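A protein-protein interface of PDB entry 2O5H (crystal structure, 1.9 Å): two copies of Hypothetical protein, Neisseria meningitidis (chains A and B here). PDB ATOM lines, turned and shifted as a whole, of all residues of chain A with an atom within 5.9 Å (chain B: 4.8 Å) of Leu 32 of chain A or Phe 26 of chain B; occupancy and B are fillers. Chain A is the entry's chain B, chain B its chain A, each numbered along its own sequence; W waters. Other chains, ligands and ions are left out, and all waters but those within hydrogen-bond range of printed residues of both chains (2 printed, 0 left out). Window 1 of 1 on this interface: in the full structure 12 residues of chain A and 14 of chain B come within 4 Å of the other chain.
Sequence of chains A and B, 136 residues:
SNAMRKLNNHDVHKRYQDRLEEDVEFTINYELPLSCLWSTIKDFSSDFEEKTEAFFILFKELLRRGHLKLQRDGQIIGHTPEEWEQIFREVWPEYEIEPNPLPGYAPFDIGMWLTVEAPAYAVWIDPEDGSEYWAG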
ATOM      1  N   PHE A  26       3.480  23.010  19.344  1.00  0.00           N
ATOM      2  CA  PHE A  26       4.594  22.307  18.694  1.00  0.00           C
ATOM      3  C   PHE A  26       5.275  23.139  17.580  1.00  0.00           C
ATOM      4  O   PHE A  26       6.504  23.275  17.582  1.00  0.00           O
ATOM      5  CB  PHE A  26       4.123  20.997  18.064  1.00  0.00           C
ATOM      6  CG  PHE A  26       4.225  19.805  18.972  1.00  0.00           C
ATOM      7  CD1 PHE A  26       3.080  19.125  19.361  1.00  0.00           C
ATOM      8  CD2 PHE A  26       5.477  19.325  19.380  1.00  0.00           C
ATOM      9  CE1 PHE A  26       3.177  17.985  20.197  1.00  0.00           C
ATOM     10  CE2 PHE A  26       5.590  18.190  20.210  1.00  0.00           C
ATOM     11  CZ  PHE A  26       4.436  17.518  20.614  1.00  0.00           C
ATOM     12  N   THR A  27       4.492  23.658  16.623  1.00  0.00           N
ATOM     13  CA  THR A  27       5.081  24.187  15.364  1.00  0.00           C
ATOM     14  C   THR A  27       5.574  25.630  15.478  1.00  0.00           C
ATOM     15  O   THR A  27       6.464  26.034  14.727  1.00  0.00           O
ATOM     16  CB  THR A  27       4.107  24.168  14.164  1.00  0.00           C
ATOM     17  OG1 THR A  27       2.943  24.949  14.490  1.00  0.00           O
ATOM     18  CG2 THR A  27       3.705  22.739  13.779  1.00  0.00           C
ATOM     19  N   TYR A  30       9.361  26.355  15.460  1.00  0.00           N
ATOM     20  CA  TYR A  30      10.232  25.935  14.381  1.00  0.00           C
ATOM     21  C   TYR A  30      10.079  26.849  13.190  1.00  0.00           C
ATOM     22  O   TYR A  30       9.160  27.676  13.153  1.00  0.00           O
ATOM     23  CB  TYR A  30       9.919  24.495  13.993  1.00  0.00           C
ATOM     24  CG  TYR A  30      10.300  23.523  15.078  1.00  0.00           C
ATOM     25  CD1 TYR A  30      11.662  23.187  15.297  1.00  0.00           C
ATOM     26  CD2 TYR A  30       9.343  22.930  15.883  1.00  0.00           C
ATOM     27  CE1 TYR A  30      12.044  22.309  16.288  1.00  0.00           C
ATOM     28  CE2 TYR A  30       9.730  22.028  16.917  1.00  0.00           C
ATOM     29  CZ  TYR A  30      11.069  21.722  17.092  1.00  0.00           C
ATOM     30  OH  TYR A  30      11.480  20.839  18.045  1.00  0.00           O
ATOM     31  N   GLU A  31      10.980  26.722  12.229  1.00  0.00           N
ATOM     32  CA  GLU A  31      10.849  27.519  11.023  1.00  0.00           C
ATOM     33  C   GLU A  31      10.379  26.641   9.879  1.00  0.00           C
ATOM     34  O   GLU A  31      11.137  26.335   9.007  1.00  0.00           O
ATOM     35  CB  GLU A  31      12.148  28.218  10.693  1.00  0.00           C
ATOM     36  CG  GLU A  31      12.448  29.343  11.661  1.00  0.00           C
ATOM     37  CD  GLU A  31      13.813  29.978  11.404  1.00  0.00           C
ATOM     38  OE1 GLU A  31      14.491  29.599  10.419  1.00  0.00           O
ATOM     39  OE2 GLU A  31      14.191  30.859  12.201  1.00  0.00           O
ATOM     40  N   LEU A  32       9.116  26.251   9.888  1.00  0.00           N
ATOM     41  CA  LEU A  32       8.670  25.225   8.940  1.00  0.00           C
ATOM     42  C   LEU A  32       8.102  25.823   7.689  1.00  0.00           C
ATOM     43  O   LEU A  32       7.254  26.704   7.783  1.00  0.00           O
ATOM     44  CB  LEU A  32       7.603  24.325   9.562  1.00  0.00           C
ATOM     45  CG  LEU A  32       8.010  23.668  10.867  1.00  0.00           C
ATOM     46  CD1 LEU A  32       6.744  23.115  11.506  1.00  0.00           C
ATOM     47  CD2 LEU A  32       9.106  22.598  10.655  1.00  0.00           C
ATOM     48  N   PRO A  33       8.493  25.283   6.513  1.00  0.00           N
ATOM     49  CA  PRO A  33       7.839  25.701   5.283  1.00  0.00           C
ATOM     50  C   PRO A  33       6.431  25.170   5.222  1.00  0.00           C
ATOM     51  O   PRO A  33       6.089  24.237   5.946  1.00  0.00           O
ATOM     52  CB  PRO A  33       8.652  25.046   4.165  1.00  0.00           C
ATOM     53  CG  PRO A  33       9.541  24.040   4.834  1.00  0.00           C
ATOM     54  CD  PRO A  33       9.566  24.293   6.312  1.00  0.00           C
ATOM     55  N   LEU A  34       5.614  25.715   4.319  1.00  0.00           N
ATOM     56  CA  LEU A  34       4.252  25.250   4.266  1.00  0.00           C
ATOM     57  C   LEU A  34       4.137  23.750   3.962  1.00  0.00           C
ATOM     58  O   LEU A  34       3.210  23.122   4.420  1.00  0.00           O
ATOM     59  CB  LEU A  34       3.403  26.056   3.293  1.00  0.00           C
ATOM     60  CG  LEU A  34       3.403  27.581   3.542  1.00  0.00           C
ATOM     61  CD1 LEU A  34       2.406  28.278   2.619  1.00  0.00           C
ATOM     62  CD2 LEU A  34       3.059  27.915   4.982  1.00  0.00           C
ATOM     63  N   CYS A  36       5.897  21.404   5.087  1.00  0.00           N
ATOM     64  CA  CYS A  36       5.982  20.782   6.410  1.00  0.00           C
ATOM     65  C   CYS A  36       4.769  20.951   7.346  1.00  0.00           C
ATOM     66  O   CYS A  36       4.430  20.031   8.103  1.00  0.00           O
ATOM     67  CB  CYS A  36       7.290  21.180   7.110  1.00  0.00           C
ATOM     68  SG  CYS A  36       8.760  20.486   6.246  1.00  0.00           S
ATOM     69  N   LEU A  37       4.121  22.116   7.316  1.00  0.00           N
ATOM     70  CA  LEU A  37       2.816  22.265   7.928  1.00  0.00           C
ATOM     71  C   LEU A  37       1.822  21.289   7.368  1.00  0.00           C
ATOM     72  O   LEU A  37       1.039  20.701   8.124  1.00  0.00           O
ATOM     73  CB  LEU A  37       2.261  23.701   7.756  1.00  0.00           C
ATOM     74  CG  LEU A  37       3.102  24.786   8.434  1.00  0.00           C
ATOM     75  CD1 LEU A  37       2.405  26.172   8.270  1.00  0.00           C
ATOM     76  CD2 LEU A  37       3.361  24.483   9.944  1.00  0.00           C
ATOM     77  N   THR A  40       2.385  18.047   8.935  1.00  0.00           N
ATOM     78  CA  THR A  40       1.993  17.942  10.339  1.00  0.00           C
ATOM     79  C   THR A  40       0.483  17.624  10.517  1.00  0.00           C
ATOM     80  O   THR A  40       0.098  16.970  11.488  1.00  0.00           O
ATOM     81  CB  THR A  40       2.340  19.206  11.162  1.00  0.00           C
ATOM     82  OG1 THR A  40       1.519  20.293  10.745  1.00  0.00           O
ATOM     83  CG2 THR A  40       3.782  19.616  10.966  1.00  0.00           C
ATOM     84  N   LEU A  68       5.159  33.595  11.283  1.00  0.00           N
ATOM     85  CA  LEU A  68       5.041  33.171   9.885  1.00  0.00           C
ATOM     86  C   LEU A  68       4.807  34.358   8.955  1.00  0.00           C
ATOM     87  O   LEU A  68       3.780  35.004   9.013  1.00  0.00           O
ATOM     88  CB  LEU A  68       3.915  32.149   9.733  1.00  0.00           C
ATOM     89  CG  LEU A  68       3.706  31.563   8.336  1.00  0.00           C
ATOM     90  CD1 LEU A  68       5.027  30.918   7.823  1.00  0.00           C
ATOM     91  CD2 LEU A  68       2.595  30.535   8.331  1.00  0.00           C
ATOM     92  N   ALA A 122       7.089  30.532   3.023  1.00  0.00           N
ATOM     93  CA  ALA A 122       7.469  30.952   4.382  1.00  0.00           C
ATOM     94  C   ALA A 122       8.873  31.539   4.427  1.00  0.00           C
ATOM     95  O   ALA A 122       9.822  30.992   3.831  1.00  0.00           O
ATOM     96  CB  ALA A 122       7.350  29.770   5.354  1.00  0.00           C
ATOM     97  N   TRP A 124      11.605  33.940   7.406  1.00  0.00           N
ATOM     98  CA  TRP A 124      11.705  34.479   8.791  1.00  0.00           C
ATOM     99  C   TRP A 124      12.515  35.772   8.962  1.00  0.00           C
ATOM    100  O   TRP A 124      13.483  36.019   8.244  1.00  0.00           O
ATOM    101  CB  TRP A 124      12.180  33.391   9.764  1.00  0.00           C
ATOM    102  CG  TRP A 124      11.024  32.596  10.246  1.00  0.00           C
ATOM    103  CD1 TRP A 124      10.325  32.802  11.390  1.00  0.00           C
ATOM    104  CD2 TRP A 124      10.401  31.499   9.581  1.00  0.00           C
ATOM    105  NE1 TRP A 124       9.304  31.892  11.492  1.00  0.00           N
ATOM    106  CE2 TRP A 124       9.328  31.079  10.391  1.00  0.00           C
ATOM    107  CE3 TRP A 124      10.644  30.822   8.374  1.00  0.00           C
ATOM    108  CZ2 TRP A 124       8.501  30.020  10.043  1.00  0.00           C
ATOM    109  CZ3 TRP A 124       9.814  29.762   8.034  1.00  0.00           C
ATOM    110  CH2 TRP A 124       8.757  29.376   8.865  1.00  0.00           C
ATOM    111  N   GLU B  22      13.687  17.640  22.423  1.00  0.00           N
ATOM    112  CA  GLU B  22      12.576  18.412  21.908  1.00  0.00           C
ATOM    113  C   GLU B  22      12.398  18.142  20.404  1.00  0.00           C
ATOM    114  O   GLU B  22      11.258  17.981  19.905  1.00  0.00           O
ATOM    115  CB  GLU B  22      12.875  19.887  22.147  1.00  0.00           C
ATOM    116  CG  GLU B  22      11.653  20.750  22.393  1.00  0.00           C
ATOM    117  CD  GLU B  22      11.766  22.101  21.702  1.00  0.00           C
ATOM    118  OE1 GLU B  22      12.785  22.804  21.959  1.00  0.00           O
ATOM    119  OE2 GLU B  22      10.846  22.445  20.900  1.00  0.00           O
ATOM    120  N   ASP B  23      13.503  18.120  19.658  1.00  0.00           N
ATOM    121  CA  ASP B  23      13.432  17.881  18.223  1.00  0.00           C
ATOM    122  C   ASP B  23      13.011  16.435  17.923  1.00  0.00           C
ATOM    123  O   ASP B  23      12.257  16.189  17.006  1.00  0.00           O
ATOM    124  CB  ASP B  23      14.792  18.205  17.546  1.00  0.00           C
ATOM    125  CG  ASP B  23      15.065  19.722  17.450  1.00  0.00           C
ATOM    126  OD1 ASP B  23      14.188  20.517  17.852  1.00  0.00           O
ATOM    127  OD2 ASP B  23      16.161  20.116  16.977  1.00  0.00           O
ATOM    128  N   VAL B  24      13.532  15.484  18.702  1.00  0.00           N
ATOM    129  CA  VAL B  24      13.081  14.096  18.664  1.00  0.00           C
ATOM    130  C   VAL B  24      11.563  13.976  18.935  1.00  0.00           C
ATOM    131  O   VAL B  24      10.831  13.389  18.130  1.00  0.00           O
ATOM    132  CB  VAL B  24      13.943  13.167  19.597  1.00  0.00           C
ATOM    133  CG1 VAL B  24      13.284  11.797  19.786  1.00  0.00           C
ATOM    134  CG2 VAL B  24      15.348  12.995  18.998  1.00  0.00           C
ATOM    135  N   GLU B  25      11.119  14.563  20.047  1.00  0.00           N
ATOM    136  CA  GLU B  25       9.704  14.602  20.409  1.00  0.00           C
ATOM    137  C   GLU B  25       8.847  15.098  19.229  1.00  0.00           C
ATOM    138  O   GLU B  25       7.916  14.411  18.785  1.00  0.00           O
ATOM    139  CB  GLU B  25       9.508  15.443  21.683  1.00  0.00           C
ATOM    140  CG  GLU B  25      10.018  14.742  22.974  1.00  0.00           C
ATOM    141  CD  GLU B  25      10.283  15.680  24.164  1.00  0.00           C
ATOM    142  OE1 GLU B  25       9.754  16.798  24.203  1.00  0.00           O
ATOM    143  OE2 GLU B  25      11.048  15.294  25.072  1.00  0.00           O
ATOM    144  N   PHE B  26       9.228  16.251  18.678  1.00  0.00           N
ATOM    145  CA  PHE B  26       8.489  16.910  17.591  1.00  0.00           C
ATOM    146  C   PHE B  26       8.381  16.008  16.344  1.00  0.00           C
ATOM    147  O   PHE B  26       7.296  15.768  15.866  1.00  0.00           O
ATOM    148  CB  PHE B  26       9.112  18.268  17.215  1.00  0.00           C
ATOM    149  CG  PHE B  26       8.479  18.932  15.984  1.00  0.00           C
ATOM    150  CD1 PHE B  26       7.143  19.389  16.030  1.00  0.00           C
ATOM    151  CD2 PHE B  26       9.229  19.115  14.810  1.00  0.00           C
ATOM    152  CE1 PHE B  26       6.551  19.993  14.900  1.00  0.00           C
ATOM    153  CE2 PHE B  26       8.645  19.743  13.677  1.00  0.00           C
ATOM    154  CZ  PHE B  26       7.300  20.177  13.734  1.00  0.00           C
ATOM    155  N   THR B  27       9.505  15.473  15.870  1.00  0.00           N
ATOM    156  CA  THR B  27       9.527  14.678  14.621  1.00  0.00           C
ATOM    157  C   THR B  27       8.826  13.293  14.794  1.00  0.00           C
ATOM    158  O   THR B  27       8.168  12.803  13.871  1.00  0.00           O
ATOM    159  CB  THR B  27      10.982  14.514  14.119  1.00  0.00           C
ATOM    160  OG1 THR B  27      11.749  13.969  15.194  1.00  0.00           O
ATOM    161  CG2 THR B  27      11.567  15.908  13.728  1.00  0.00           C
ATOM    162  N   ILE B  28       8.949  12.682  15.975  1.00  0.00           N
ATOM    163  CA  ILE B  28       8.202  11.437  16.288  1.00  0.00           C
ATOM    164  C   ILE B  28       6.699  11.724  16.266  1.00  0.00           C
ATOM    165  O   ILE B  28       5.893  10.976  15.668  1.00  0.00           O
ATOM    166  CB  ILE B  28       8.577  10.873  17.713  1.00  0.00           C
ATOM    167  CG1 ILE B  28      10.007  10.330  17.742  1.00  0.00           C
ATOM    168  CG2 ILE B  28       7.529   9.825  18.206  1.00  0.00           C
ATOM    169  CD1 ILE B  28      10.503  10.107  19.187  1.00  0.00           C
ATOM    170  N   ASN B  29       6.304  12.825  16.895  1.00  0.00           N
ATOM    171  CA  ASN B  29       4.874  13.135  16.977  1.00  0.00           C
ATOM    172  C   ASN B  29       4.167  13.234  15.632  1.00  0.00           C
ATOM    173  O   ASN B  29       3.057  12.761  15.490  1.00  0.00           O
ATOM    174  CB  ASN B  29       4.593  14.403  17.775  1.00  0.00           C
ATOM    175  CG  ASN B  29       3.114  14.557  18.093  1.00  0.00           C
ATOM    176  OD1 ASN B  29       2.544  13.748  18.817  1.00  0.00           O
ATOM    177  ND2 ASN B  29       2.475  15.569  17.512  1.00  0.00           N
ATOM    178  N   TYR B  30       4.821  13.832  14.649  1.00  0.00           N
ATOM    179  CA  TYR B  30       4.178  14.093  13.368  1.00  0.00           C
ATOM    180  C   TYR B  30       4.654  13.199  12.240  1.00  0.00           C
ATOM    181  O   TYR B  30       4.205  13.346  11.100  1.00  0.00           O
ATOM    182  CB  TYR B  30       4.362  15.568  12.989  1.00  0.00           C
ATOM    183  CG  TYR B  30       3.594  16.473  13.934  1.00  0.00           C
ATOM    184  CD1 TYR B  30       2.195  16.503  13.922  1.00  0.00           C
ATOM    185  CD2 TYR B  30       4.265  17.262  14.845  1.00  0.00           C
ATOM    186  CE1 TYR B  30       1.477  17.311  14.812  1.00  0.00           C
ATOM    187  CE2 TYR B  30       3.569  18.082  15.740  1.00  0.00           C
ATOM    188  CZ  TYR B  30       2.179  18.097  15.717  1.00  0.00           C
ATOM    189  OH  TYR B  30       1.494  18.903  16.593  1.00  0.00           O
ATOM    190  N   LEU B  32       7.441  13.013  10.486  1.00  0.00           N
ATOM    191  CA  LEU B  32       7.878  13.944   9.441  1.00  0.00           C
ATOM    192  C   LEU B  32       8.899  13.305   8.476  1.00  0.00           C
ATOM    193  O   LEU B  32       9.757  12.550   8.918  1.00  0.00           O
ATOM    194  CB  LEU B  32       8.505  15.198  10.113  1.00  0.00           C
ATOM    195  CG  LEU B  32       7.484  16.089  10.861  1.00  0.00           C
ATOM    196  CD1 LEU B  32       8.207  17.301  11.474  1.00  0.00           C
ATOM    197  CD2 LEU B  32       6.387  16.539   9.888  1.00  0.00           C
ATOM    198  N   CYS B  36      11.609  17.498   6.276  1.00  0.00           N
ATOM    199  CA  CYS B  36      11.090  18.261   7.431  1.00  0.00           C
ATOM    200  C   CYS B  36      11.967  18.100   8.663  1.00  0.00           C
ATOM    201  O   CYS B  36      11.898  18.935   9.572  1.00  0.00           O
ATOM    202  CB  CYS B  36       9.605  17.923   7.723  1.00  0.00           C
ATOM    203  SG  CYS B  36       8.516  18.385   6.368  1.00  0.00           S
ATOM    204  N   SER B  39      14.056  21.047   8.033  1.00  0.00           N
ATOM    205  CA  SER B  39      13.316  22.237   8.478  1.00  0.00           C
ATOM    206  C   SER B  39      13.294  22.390  10.029  1.00  0.00           C
ATOM    207  O   SER B  39      13.399  23.500  10.550  1.00  0.00           O
ATOM    208  CB  SER B  39      11.907  22.213   7.909  1.00  0.00           C
ATOM    209  OG  SER B  39      11.989  22.255   6.488  1.00  0.00           O
ATOM    210  N   THR B  40      13.183  21.271  10.738  1.00  0.00           N
ATOM    211  CA  THR B  40      13.201  21.237  12.201  1.00  0.00           C
ATOM    212  C   THR B  40      14.484  21.825  12.811  1.00  0.00           C
ATOM    213  O   THR B  40      14.443  22.507  13.863  1.00  0.00           O
ATOM    214  CB  THR B  40      13.010  19.757  12.706  1.00  0.00           C
ATOM    215  OG1 THR B  40      11.746  19.238  12.254  1.00  0.00           O
ATOM    216  CG2 THR B  40      13.052  19.671  14.235  1.00  0.00           C
HETATM  217  O   HOH W   1      13.379  25.269  12.618  1.00  0.00           O
HETATM  218  O   HOH W   2       7.835  22.269  19.997  1.00  0.00           O
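Leu 32 of chain A touches just these residues of chain B: Phe 26 and Ser 39. Of chain A, only Phe 26, Tyr 30 and Leu 32 come within 4 Å of Phe 26 of chain B. Of the printed residues of chain A, Ser 39 of chain B touches Glu 31 (3.9 Å), Leu 32 (3.9 Å), Pro 33 (3.2 Å) and Cys 36 (3.7 Å). Of the printed residues of chain A, Thr 40 of chain B touches Tyr 30 (3.2 Å). Printed residues of chain B within 4 Å of Thr 40 of chain A: Tyr 30. Of the printed residues of chain B, Tyr 30 of chain A touches Glu 22 (3.3 Å), Asp 23 (2.7 Å), Phe 26 (3.5 Å) and Thr 40 (3.2 Å). Of the printed residues of chain B, Phe 26 of chain A touches Phe 26 (3.7 Å), Asn 29 (3.7 Å) and Tyr 30 (3.2 Å). The nearest residue of chain B that does not touch Leu 32 of chain A is Thr 40 of chain B (4.3 Å).
Phe 26 of chain A touches Tyr 30 of chain B, and with the chains exchanged Tyr 30 of chain A touches Phe 26 of chain B. Tyr 30 of chain A touches Thr 40 of chain B, and with the chains exchanged Thr 40 of chain A touches Tyr 30 of chain B. Leu 32 of chain A touches Phe 26 of chain B, but with the chains exchanged Phe 26 of chain A does not touch Leu 32 of chain B (8.6 Å). Cys 36 of chain A touches its own counterpart, Cys 36 of chain B.
The side-chain hydroxyl of Ser 39 of chain B lies within hydrogen-bond range of the side-chain sulfur of Cys 36 of chain A, at 3.7 Å. The side-chain carboxylate of Asp 23 of chain B is in hydrogen-bond range of the side-chain hydroxyl of Tyr 30 of chain A (2.7 Å). OH of Tyr 30 of chain A lies within hydrogen-bond range of OE2 of Glu 22 of chain B (3.3 Å). SG of Cys 36 of chain B forms a disulfide with SG of Cys 36 of chain A (2.1 Å).
Water W1 lies within hydrogen-bond range of O of Ser 39 of chain B (2.7 Å), N of Glu 31 of chain A (2.8 Å) and O of Thr 40 of chain B (3.2 Å). Water W2 lies within hydrogen-bond range of O of Phe 26 of chain A (2.9 Å) and OE2 of Glu 22 of chain B (3.1 Å).
Among the printed residues, pairs that only touch across the chains: Pro 33 of chain A with Ser 39 of chain B (3.2 Å), Phe 26 of chain A with Tyr 30 of chain B (3.2 Å), Tyr 30 of chain A with Thr 40 of chain B (3.2 Å), Thr 40 of chain A with Tyr 30 of chain B (3.2 Å), Tyr 30 of chain A with Phe 26 of chain B (3.5 Å), Phe 26 of chain A with Asn 29 of chain B (3.7 Å), Leu 32 of chain A with Phe 26 of chain B (3.7 Å), Phe 26 of chain A with Phe 26 of chain B (3.7 Å), Leu 32 of chain A with Ser 39 of chain B (3.9 Å) and Glu 31 of chain A with Ser 39 of chain B (3.9 Å).
Hydrophobic or aromatic side chains of chain A within 4 Å of the printed part of chain B: Phe 26, Tyr 30, Leu 32 and Pro 33. Among the printed residues, 14 pairs touch across the chains.
The backbone carbonyl oxygen of Leu 37 of chain A is in hydrogen-bond range of the side-chain hydroxyl of Thr 40 of chain A. O of Cys 36 of chain B sits at hydrogen-bond distance from OG1 of Thr 40 of chain B (2.7 Å). O of Asp 23 of chain B lies within hydrogen-bond range of OG1 of Thr 27 of chain B, 2.9 Å away.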
